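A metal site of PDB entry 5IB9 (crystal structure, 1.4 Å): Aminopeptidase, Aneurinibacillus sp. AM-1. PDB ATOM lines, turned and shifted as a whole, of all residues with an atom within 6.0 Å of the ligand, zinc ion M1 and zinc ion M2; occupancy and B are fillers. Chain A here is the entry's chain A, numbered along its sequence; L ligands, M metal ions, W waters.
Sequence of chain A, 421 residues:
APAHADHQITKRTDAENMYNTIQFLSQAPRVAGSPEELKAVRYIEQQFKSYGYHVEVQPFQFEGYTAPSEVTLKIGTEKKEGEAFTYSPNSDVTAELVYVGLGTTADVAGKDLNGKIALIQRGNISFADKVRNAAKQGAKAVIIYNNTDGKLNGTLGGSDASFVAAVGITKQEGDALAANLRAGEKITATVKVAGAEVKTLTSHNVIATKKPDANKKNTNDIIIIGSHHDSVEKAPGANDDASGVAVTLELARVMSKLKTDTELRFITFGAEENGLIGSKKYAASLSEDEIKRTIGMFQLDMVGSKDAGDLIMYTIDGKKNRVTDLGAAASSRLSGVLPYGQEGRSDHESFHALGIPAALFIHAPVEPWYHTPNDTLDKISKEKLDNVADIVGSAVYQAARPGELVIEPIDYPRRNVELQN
Water W1 lies within hydrogen-bond range of O3 of the ligand (3.4 Å) and NE of Arg 345 (3.4 Å).
Zinc ion M1 is bound by the side-chain carboxylate (OD2) of Asp 240, a ring nitrogen (NE2) of His 371, an oxygen (O1) of the ligand, the side-chain carboxylate (OE2) of Glu 273, an oxygen (O2) of the ligand and the side-chain carboxylate (OE1) of Glu 273. Zinc ion M1 has six donor atoms within binding distance.
The side-chain carboxylate (OE1) of Glu 272 sits close to a ring nitrogen (NE2) of His 228. OD2 of Asp 241 sits at hydrogen-bond distance from N of His 228 (3.2 Å). The backbone carbonyl oxygen of Asp 230 sits at hydrogen-bond distance from a ring nitrogen (ND1) of His 228. The side-chain carboxylate (OD2) of Asp 301 sits close to the side-chain hydroxyl (OG) of Ser 346 (2.7 Å). The backbone NH (N) of Glu 273 is in hydrogen-bond range of the side-chain carboxylate (OD2) of Asp 230 (2.9 Å). The guanidinium group of Arg 345 is in hydrogen-bond range of the side-chain hydroxyl of Tyr 370, at 3.1 Å. The side-chain carboxylate of Glu 343 is in salt-bridge range of the guanidinium group of Arg 345 (3.8 Å). The side-chain carboxylate of Glu 349 is in hydrogen-bond range of the backbone NH of Arg 345.
The backbone carbonyl oxygen (O) of Arg 345 sits close to a nitrogen (N2) of the ligand. O4 of the ligand lies within salt-bridge range of NE of Arg 345, 2.7 Å away. OH of Tyr 370 sits at hydrogen-bond distance from O4 of the ligand (3.0 Å). The side-chain carboxylate (OE1) of Glu 272 lies close to an oxygen (O1) of the ligand. The side-chain sulfur of Met 302 sits close to a nitrogen (N1) of the ligand, at 3.5 Å.
Tyr 370 touches zinc ion M1. Within 4 Å of zinc ion M1: Asp 240, Glu 273, Tyr 370 and His 371.
OD1 of Asp 240 is bound to zinc ion M2, at 2.0 Å. A ring nitrogen (NE2) of His 228 is bound to zinc ion M2, 2.0 Å away. An oxygen (O1) of the ligand is bound to zinc ion M2, 2.1 Å away. OD1 of Asp 301 is bound to zinc ion M2, 2.1 Å away. OD2 of Asp 301 binds zinc ion M2 (2.3 Å). Zinc ion M2 is bound by N1 of the ligand.
Gly 275 touches the ligand. Leu 276 touches the ligand (CD2 to C14, 3.99 Å). CD1 of Ile 362 touches C7 of the ligand, at 3.6 Å. Val 366 touches the ligand. Hydrophobic or aromatic side chains that line the ligand: His 228, Leu 276, Met 302, Ile 362, Val 366, Tyr 370 and His 371. 13 residues have an atom within 4 Å of the ligand: His 228, Asp 240, Glu 272, Glu 273, Gly 275, Leu 276, Asp 301, Met 302, Arg 345, Ile 362, Val 366, Tyr 370 and His 371. Along chain A the residues within 4 Å of the ligand span positions 228 to 371. The nearest printed residue that does not touch the ligand is Leu 360 (4.2 Å).
Residues that only touch zinc ion M2: Asp 241 (3.97 Å) and Glu 272 (3.9 Å). Six residues have an atom within 4 Å of zinc ion M2: His 228, Asp 240, Asp 241, Glu 272, Glu 273 and Asp 301.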
ATOM      1  N   HIS A 228      17.634  -1.983 -23.673  1.00  0.00           N
ATOM      2  CA  HIS A 228      17.693  -0.547 -24.037  1.00  0.00           C
ATOM      3  C   HIS A 228      17.285  -0.313 -25.483  1.00  0.00           C
ATOM      4  O   HIS A 228      17.546  -1.168 -26.359  1.00  0.00           O
ATOM      5  CB  HIS A 228      19.124   0.090 -23.758  1.00  0.00           C
ATOM      6  CG  HIS A 228      20.258  -0.445 -24.626  1.00  0.00           C
ATOM      7  ND1 HIS A 228      20.654   0.226 -25.795  1.00  0.00           N
ATOM      8  CD2 HIS A 228      21.144  -1.411 -24.385  1.00  0.00           C
ATOM      9  CE1 HIS A 228      21.738  -0.441 -26.270  1.00  0.00           C
ATOM     10  NE2 HIS A 228      22.022  -1.436 -25.454  1.00  0.00           N
ATOM     11  N   ASP A 230      17.879   2.591 -27.360  1.00  0.00           N
ATOM     12  CA  ASP A 230      18.738   3.475 -28.194  1.00  0.00           C
ATOM     13  C   ASP A 230      19.892   2.666 -28.800  1.00  0.00           C
ATOM     14  O   ASP A 230      20.232   1.556 -28.343  1.00  0.00           O
ATOM     15  CB  ASP A 230      19.328   4.596 -27.348  1.00  0.00           C
ATOM     16  CG  ASP A 230      20.259   4.136 -26.245  1.00  0.00           C
ATOM     17  OD1 ASP A 230      19.961   3.157 -25.484  1.00  0.00           O
ATOM     18  OD2 ASP A 230      21.341   4.758 -26.118  1.00  0.00           O
ATOM     19  N   VAL A 232      23.907   3.376 -30.998  1.00  0.00           N
ATOM     20  CA  VAL A 232      24.934   4.442 -31.273  1.00  0.00           C
ATOM     21  C   VAL A 232      24.736   5.087 -32.651  1.00  0.00           C
ATOM     22  O   VAL A 232      24.067   4.533 -33.534  1.00  0.00           O
ATOM     23  CB  VAL A 232      26.354   3.845 -31.178  1.00  0.00           C
ATOM     24  CG1 VAL A 232      26.596   3.332 -29.714  1.00  0.00           C
ATOM     25  CG2 VAL A 232      26.668   2.784 -32.234  1.00  0.00           C
ATOM     26  N   ASP A 240      22.156  -4.577 -31.203  1.00  0.00           N
ATOM     27  CA  ASP A 240      22.490  -3.723 -30.061  1.00  0.00           C
ATOM     28  C   ASP A 240      21.542  -2.533 -30.125  1.00  0.00           C
ATOM     29  O   ASP A 240      21.931  -1.520 -30.694  1.00  0.00           O
ATOM     30  CB  ASP A 240      24.007  -3.223 -30.098  1.00  0.00           C
ATOM     31  CG  ASP A 240      24.468  -2.569 -28.846  1.00  0.00           C
ATOM     32  OD1 ASP A 240      23.525  -2.672 -27.832  1.00  0.00           O
ATOM     33  OD2 ASP A 240      25.517  -1.830 -28.585  1.00  0.00           O
ATOM     34  N   ASP A 241      20.305  -2.499 -29.558  1.00  0.00           N
ATOM     35  CA  ASP A 241      19.786  -3.561 -28.730  1.00  0.00           C
ATOM     36  C   ASP A 241      18.332  -3.746 -29.099  1.00  0.00           C
ATOM     37  O   ASP A 241      17.507  -4.084 -28.243  1.00  0.00           O
ATOM     38  CB  ASP A 241      19.953  -3.285 -27.231  1.00  0.00           C
ATOM     39  CG  ASP A 241      19.611  -4.526 -26.420  1.00  0.00           C
ATOM     40  OD1 ASP A 241      19.626  -5.692 -26.872  1.00  0.00           O
ATOM     41  OD2 ASP A 241      19.246  -4.292 -25.162  1.00  0.00           O
ATOM     42  N   GLU A 272      21.133   4.380 -22.946  1.00  0.00           N
ATOM     43  CA  GLU A 272      22.083   3.382 -22.470  1.00  0.00           C
ATOM     44  C   GLU A 272      23.499   3.679 -23.003  1.00  0.00           C
ATOM     45  O   GLU A 272      24.474   3.566 -22.240  1.00  0.00           O
ATOM     46  CB  GLU A 272      21.617   1.936 -22.775  1.00  0.00           C
ATOM     47  CG  GLU A 272      22.489   0.865 -22.098  1.00  0.00           C
ATOM     48  CD  GLU A 272      23.667   0.410 -22.993  1.00  0.00           C
ATOM     49  OE1 GLU A 272      23.782   0.835 -24.174  1.00  0.00           O
ATOM     50  OE2 GLU A 272      24.427  -0.375 -22.382  1.00  0.00           O
ATOM     51  N   GLU A 273      23.516   4.068 -24.275  1.00  0.00           N
ATOM     52  CA  GLU A 273      24.854   4.161 -24.931  1.00  0.00           C
ATOM     53  C   GLU A 273      25.587   5.403 -24.450  1.00  0.00           C
ATOM     54  O   GLU A 273      26.832   5.476 -24.650  1.00  0.00           O
ATOM     55  CB  GLU A 273      24.618   4.221 -26.415  1.00  0.00           C
ATOM     56  CG  GLU A 273      23.989   2.959 -27.121  1.00  0.00           C
ATOM     57  CD  GLU A 273      24.899   1.712 -27.137  1.00  0.00           C
ATOM     58  OE1 GLU A 273      26.003   1.772 -26.493  1.00  0.00           O
ATOM     59  OE2 GLU A 273      24.425   0.665 -27.778  1.00  0.00           O
ATOM     60  N   ASN A 274      24.883   6.304 -23.813  1.00  0.00           N
ATOM     61  CA  ASN A 274      25.423   7.508 -23.224  1.00  0.00           C
ATOM     62  C   ASN A 274      25.963   7.356 -21.820  1.00  0.00           C
ATOM     63  O   ASN A 274      26.278   8.358 -21.173  1.00  0.00           O
ATOM     64  CB  ASN A 274      24.297   8.637 -23.165  1.00  0.00           C
ATOM     65  CG  ASN A 274      23.651   8.885 -24.530  1.00  0.00           C
ATOM     66  OD1 ASN A 274      24.038   9.814 -25.267  1.00  0.00           O
ATOM     67  ND2 ASN A 274      22.796   7.968 -24.931  1.00  0.00           N
ATOM     68  N   GLY A 275      25.991   6.128 -21.264  1.00  0.00           N
ATOM     69  CA  GLY A 275      26.414   5.897 -19.932  1.00  0.00           C
ATOM     70  C   GLY A 275      25.304   5.431 -18.997  1.00  0.00           C
ATOM     71  O   GLY A 275      25.289   5.738 -17.821  1.00  0.00           O
ATOM     72  N   LEU A 276      24.426   4.566 -19.508  1.00  0.00           N
ATOM     73  CA  LEU A 276      23.380   3.934 -18.678  1.00  0.00           C
ATOM     74  C   LEU A 276      22.426   4.965 -18.144  1.00  0.00           C
ATOM     75  O   LEU A 276      21.983   4.788 -17.000  1.00  0.00           O
ATOM     76  CB  LEU A 276      23.966   2.995 -17.573  1.00  0.00           C
ATOM     77  CG  LEU A 276      25.140   2.123 -18.046  1.00  0.00           C
ATOM     78  CD1 LEU A 276      25.544   1.295 -16.819  1.00  0.00           C
ATOM     79  CD2 LEU A 276      24.845   1.249 -19.237  1.00  0.00           C
ATOM     80  N   ASP A 301      20.742  -7.754 -23.648  1.00  0.00           N
ATOM     81  CA  ASP A 301      21.489  -6.798 -24.581  1.00  0.00           C
ATOM     82  C   ASP A 301      22.342  -7.687 -25.483  1.00  0.00           C
ATOM     83  O   ASP A 301      23.234  -8.389 -24.985  1.00  0.00           O
ATOM     84  CB  ASP A 301      22.349  -5.946 -23.701  1.00  0.00           C
ATOM     85  CG  ASP A 301      22.864  -4.635 -24.402  1.00  0.00           C
ATOM     86  OD1 ASP A 301      22.692  -4.534 -25.622  1.00  0.00           O
ATOM     87  OD2 ASP A 301      23.305  -3.656 -23.767  1.00  0.00           O
ATOM     88  N   MET A 302      22.070  -7.572 -26.771  1.00  0.00           N
ATOM     89  CA  MET A 302      22.698  -8.347 -27.834  1.00  0.00           C
ATOM     90  C   MET A 302      22.428  -9.828 -27.736  1.00  0.00           C
ATOM     91  O   MET A 302      23.272 -10.574 -27.340  1.00  0.00           O
ATOM     92  CB  MET A 302      24.172  -8.004 -27.891  1.00  0.00           C
ATOM     93  CG  MET A 302      24.321  -6.639 -28.297  1.00  0.00           C
ATOM     94  SD  MET A 302      25.998  -5.906 -28.252  1.00  0.00           S
ATOM     95  CE  MET A 302      26.900  -7.041 -29.274  1.00  0.00           C
ATOM     96  N   TYR A 314      26.446 -12.321 -17.473  1.00  0.00           N
ATOM     97  CA  TYR A 314      27.511 -11.554 -16.852  1.00  0.00           C
ATOM     98  C   TYR A 314      26.989 -10.820 -15.625  1.00  0.00           C
ATOM     99  O   TYR A 314      25.911 -10.208 -15.618  1.00  0.00           O
ATOM    100  CB  TYR A 314      28.009 -10.488 -17.803  1.00  0.00           C
ATOM    101  CG  TYR A 314      28.972 -10.977 -18.873  1.00  0.00           C
ATOM    102  CD1 TYR A 314      30.042 -11.780 -18.570  1.00  0.00           C
ATOM    103  CD2 TYR A 314      28.742 -10.631 -20.185  1.00  0.00           C
ATOM    104  CE1 TYR A 314      30.905 -12.233 -19.632  1.00  0.00           C
ATOM    105  CE2 TYR A 314      29.622 -11.078 -21.270  1.00  0.00           C
ATOM    106  CZ  TYR A 314      30.691 -11.830 -20.935  1.00  0.00           C
ATOM    107  OH  TYR A 314      31.543 -12.325 -21.927  1.00  0.00           O
ATOM    108  N   GLU A 343      31.123  -8.894 -16.165  1.00  0.00           N
ATOM    109  CA  GLU A 343      31.161  -7.794 -17.058  1.00  0.00           C
ATOM    110  C   GLU A 343      30.044  -6.819 -16.657  1.00  0.00           C
ATOM    111  O   GLU A 343      28.976  -7.237 -16.180  1.00  0.00           O
ATOM    112  CB  GLU A 343      30.977  -8.236 -18.515  1.00  0.00           C
ATOM    113  CG  GLU A 343      31.059  -7.137 -19.501  1.00  0.00           C
ATOM    114  CD  GLU A 343      32.405  -6.380 -19.493  1.00  0.00           C
ATOM    115  OE1 GLU A 343      33.225  -6.752 -20.394  1.00  0.00           O
ATOM    116  OE2 GLU A 343      32.583  -5.450 -18.643  1.00  0.00           O
ATOM    117  N   GLY A 344      30.315  -5.571 -16.916  1.00  0.00           N
ATOM    118  CA  GLY A 344      29.382  -4.438 -16.716  1.00  0.00           C
ATOM    119  C   GLY A 344      28.882  -4.007 -18.121  1.00  0.00           C
ATOM    120  O   GLY A 344      28.539  -4.846 -18.970  1.00  0.00           O
ATOM    121  N   ARG A 345      28.896  -2.706 -18.357  1.00  0.00           N
ATOM    122  CA  ARG A 345      28.699  -2.111 -19.685  1.00  0.00           C
ATOM    123  C   ARG A 345      27.260  -2.190 -20.176  1.00  0.00           C
ATOM    124  O   ARG A 345      27.021  -2.119 -21.418  1.00  0.00           O
ATOM    125  CB  ARG A 345      29.624  -2.709 -20.795  1.00  0.00           C
ATOM    126  CG  ARG A 345      31.130  -2.652 -20.476  1.00  0.00           C
ATOM    127  CD  ARG A 345      31.966  -3.577 -21.472  1.00  0.00           C
ATOM    128  NE  ARG A 345      31.839  -3.149 -22.865  1.00  0.00           N
ATOM    129  CZ  ARG A 345      32.420  -3.748 -23.896  1.00  0.00           C
ATOM    130  NH1 ARG A 345      33.225  -4.790 -23.699  1.00  0.00           N
ATOM    131  NH2 ARG A 345      32.221  -3.291 -25.128  1.00  0.00           N
ATOM    132  N   SER A 346      26.300  -2.457 -19.264  1.00  0.00           N
ATOM    133  CA  SER A 346      24.839  -2.460 -19.707  1.00  0.00           C
ATOM    134  C   SER A 346      24.030  -2.157 -18.448  1.00  0.00           C
ATOM    135  O   SER A 346      24.564  -1.957 -17.393  1.00  0.00           O
ATOM    136  CB  SER A 346      24.446  -3.770 -20.397  1.00  0.00           C
ATOM    137  OG  SER A 346      23.233  -3.589 -21.109  1.00  0.00           O
ATOM    138  N   GLU A 349      24.135  -2.919 -14.470  1.00  0.00           N
ATOM    139  CA  GLU A 349      24.996  -2.171 -13.510  1.00  0.00           C
ATOM    140  C   GLU A 349      24.225  -1.198 -12.669  1.00  0.00           C
ATOM    141  O   GLU A 349      24.633  -0.897 -11.544  1.00  0.00           O
ATOM    142  CB  GLU A 349      26.016  -1.423 -14.318  1.00  0.00           C
ATOM    143  CG  GLU A 349      27.218  -0.903 -13.467  1.00  0.00           C
ATOM    144  CD  GLU A 349      28.361  -0.476 -14.407  1.00  0.00           C
ATOM    145  OE1 GLU A 349      28.837  -1.242 -15.291  1.00  0.00           O
ATOM    146  OE2 GLU A 349      28.755   0.658 -14.276  1.00  0.00           O
ATOM    147  N   LEU A 360      23.375  -9.686 -16.955  1.00  0.00           N
ATOM    148  CA  LEU A 360      23.245  -9.433 -18.408  1.00  0.00           C
ATOM    149  C   LEU A 360      23.305 -10.750 -19.110  1.00  0.00           C
ATOM    150  O   LEU A 360      24.223 -11.596 -18.893  1.00  0.00           O
ATOM    151  CB  LEU A 360      24.408  -8.539 -18.802  1.00  0.00           C
ATOM    152  CG  LEU A 360      24.643  -8.501 -20.307  1.00  0.00           C
ATOM    153  CD1 LEU A 360      23.451  -7.896 -21.148  1.00  0.00           C
ATOM    154  CD2 LEU A 360      25.969  -7.654 -20.630  1.00  0.00           C
ATOM    155  N   ILE A 362      23.721 -12.191 -22.931  1.00  0.00           N
ATOM    156  CA  ILE A 362      24.338 -11.674 -24.196  1.00  0.00           C
ATOM    157  C   ILE A 362      25.041 -12.843 -24.835  1.00  0.00           C
ATOM    158  O   ILE A 362      25.430 -13.805 -24.122  1.00  0.00           O
ATOM    159  CB  ILE A 362      25.354 -10.602 -23.841  1.00  0.00           C
ATOM    160  CG1 ILE A 362      25.989 -10.020 -25.129  1.00  0.00           C
ATOM    161  CG2 ILE A 362      26.393 -11.044 -22.798  1.00  0.00           C
ATOM    162  CD1 ILE A 362      26.658  -8.612 -24.847  1.00  0.00           C
ATOM    163  N   VAL A 366      31.127 -11.258 -28.885  1.00  0.00           N
ATOM    164  CA  VAL A 366      30.174 -10.507 -29.673  1.00  0.00           C
ATOM    165  C   VAL A 366      30.600 -10.495 -31.152  1.00  0.00           C
ATOM    166  O   VAL A 366      31.777 -10.694 -31.503  1.00  0.00           O
ATOM    167  CB  VAL A 366      29.933  -9.074 -29.207  1.00  0.00           C
ATOM    168  CG1 VAL A 366      29.514  -9.060 -27.661  1.00  0.00           C
ATOM    169  CG2 VAL A 366      31.134  -8.126 -29.460  1.00  0.00           C
ATOM    170  N   TYR A 370      29.006  -5.014 -34.052  1.00  0.00           N
ATOM    171  CA  TYR A 370      28.716  -4.240 -32.905  1.00  0.00           C
ATOM    172  C   TYR A 370      29.107  -2.745 -33.063  1.00  0.00           C
ATOM    173  O   TYR A 370      30.242  -2.484 -33.372  1.00  0.00           O
ATOM    174  CB  TYR A 370      29.572  -4.947 -31.835  1.00  0.00           C
ATOM    175  CG  TYR A 370      29.673  -4.217 -30.547  1.00  0.00           C
ATOM    176  CD1 TYR A 370      28.561  -3.893 -29.846  1.00  0.00           C
ATOM    177  CD2 TYR A 370      30.924  -3.891 -30.009  1.00  0.00           C
ATOM    178  CE1 TYR A 370      28.634  -3.214 -28.629  1.00  0.00           C
ATOM    179  CE2 TYR A 370      31.023  -3.221 -28.803  1.00  0.00           C
ATOM    180  CZ  TYR A 370      29.854  -2.865 -28.135  1.00  0.00           C
ATOM    181  OH  TYR A 370      29.939  -2.191 -26.928  1.00  0.00           O
ATOM    182  N   HIS A 371      28.192  -1.782 -32.904  1.00  0.00           N
ATOM    183  CA  HIS A 371      28.445  -0.362 -32.959  1.00  0.00           C
ATOM    184  C   HIS A 371      28.823   0.110 -34.366  1.00  0.00           C
ATOM    185  O   HIS A 371      29.324   1.209 -34.489  1.00  0.00           O
ATOM    186  CB  HIS A 371      29.407   0.109 -31.894  1.00  0.00           C
ATOM    187  CG  HIS A 371      28.790   0.125 -30.501  1.00  0.00           C
ATOM    188  ND1 HIS A 371      29.451   0.624 -29.415  1.00  0.00           N
ATOM    189  CD2 HIS A 371      27.603  -0.376 -30.044  1.00  0.00           C
ATOM    190  CE1 HIS A 371      28.671   0.478 -28.320  1.00  0.00           C
ATOM    191  NE2 HIS A 371      27.571  -0.156 -28.688  1.00  0.00           N
HETATM  192  N1  LIG L   1      25.790  -3.943 -25.400  1.00  0.00           N
HETATM  193  C1  LIG L   1      26.844  -3.000 -25.045  1.00  0.00           C
HETATM  194  C2  LIG L   1      27.693  -3.624 -23.938  1.00  0.00           C
HETATM  195  C3  LIG L   1      28.572  -4.822 -24.287  1.00  0.00           C
HETATM  196  C4  LIG L   1      29.288  -4.929 -25.505  1.00  0.00           C
HETATM  197  C5  LIG L   1      28.710  -5.843 -23.316  1.00  0.00           C
HETATM  198  C6  LIG L   1      30.116  -6.045 -25.733  1.00  0.00           C
HETATM  199  C7  LIG L   1      29.534  -6.975 -23.551  1.00  0.00           C
HETATM  200  C8  LIG L   1      30.231  -7.069 -24.771  1.00  0.00           C
HETATM  201  C9  LIG L   1      26.243  -1.673 -24.602  1.00  0.00           C
HETATM  202  O1  LIG L   1      25.269  -1.446 -25.620  1.00  0.00           O
HETATM  203  C10 LIG L   1      27.347  -0.677 -24.706  1.00  0.00           C
HETATM  204  O2  LIG L   1      27.783  -0.418 -25.823  1.00  0.00           O
HETATM  205  N2  LIG L   1      27.839  -0.205 -23.616  1.00  0.00           N
HETATM  206  C11 LIG L   1      28.981   0.716 -23.668  1.00  0.00           C
HETATM  207  C12 LIG L   1      29.241   1.039 -22.214  1.00  0.00           C
HETATM  208  C13 LIG L   1      28.097   1.776 -21.504  1.00  0.00           C
HETATM  209  C14 LIG L   1      28.644   2.102 -20.126  1.00  0.00           C
HETATM  210  C15 LIG L   1      27.573   3.017 -22.240  1.00  0.00           C
HETATM  211  C16 LIG L   1      30.265   0.057 -24.155  1.00  0.00           C
HETATM  212  O3  LIG L   1      31.202   0.795 -24.561  1.00  0.00           O
HETATM  213  O4  LIG L   1      30.422  -1.180 -24.154  1.00  0.00           O
HETATM  214 ZN    ZN M   1      26.039  -0.640 -27.403  1.00  0.00          ZN
HETATM  215 ZN    ZN M   2      23.609  -2.648 -25.826  1.00  0.00          ZN
HETATM  216  O   HOH W   1      33.260  -0.164 -22.042  1.00  0.00           O
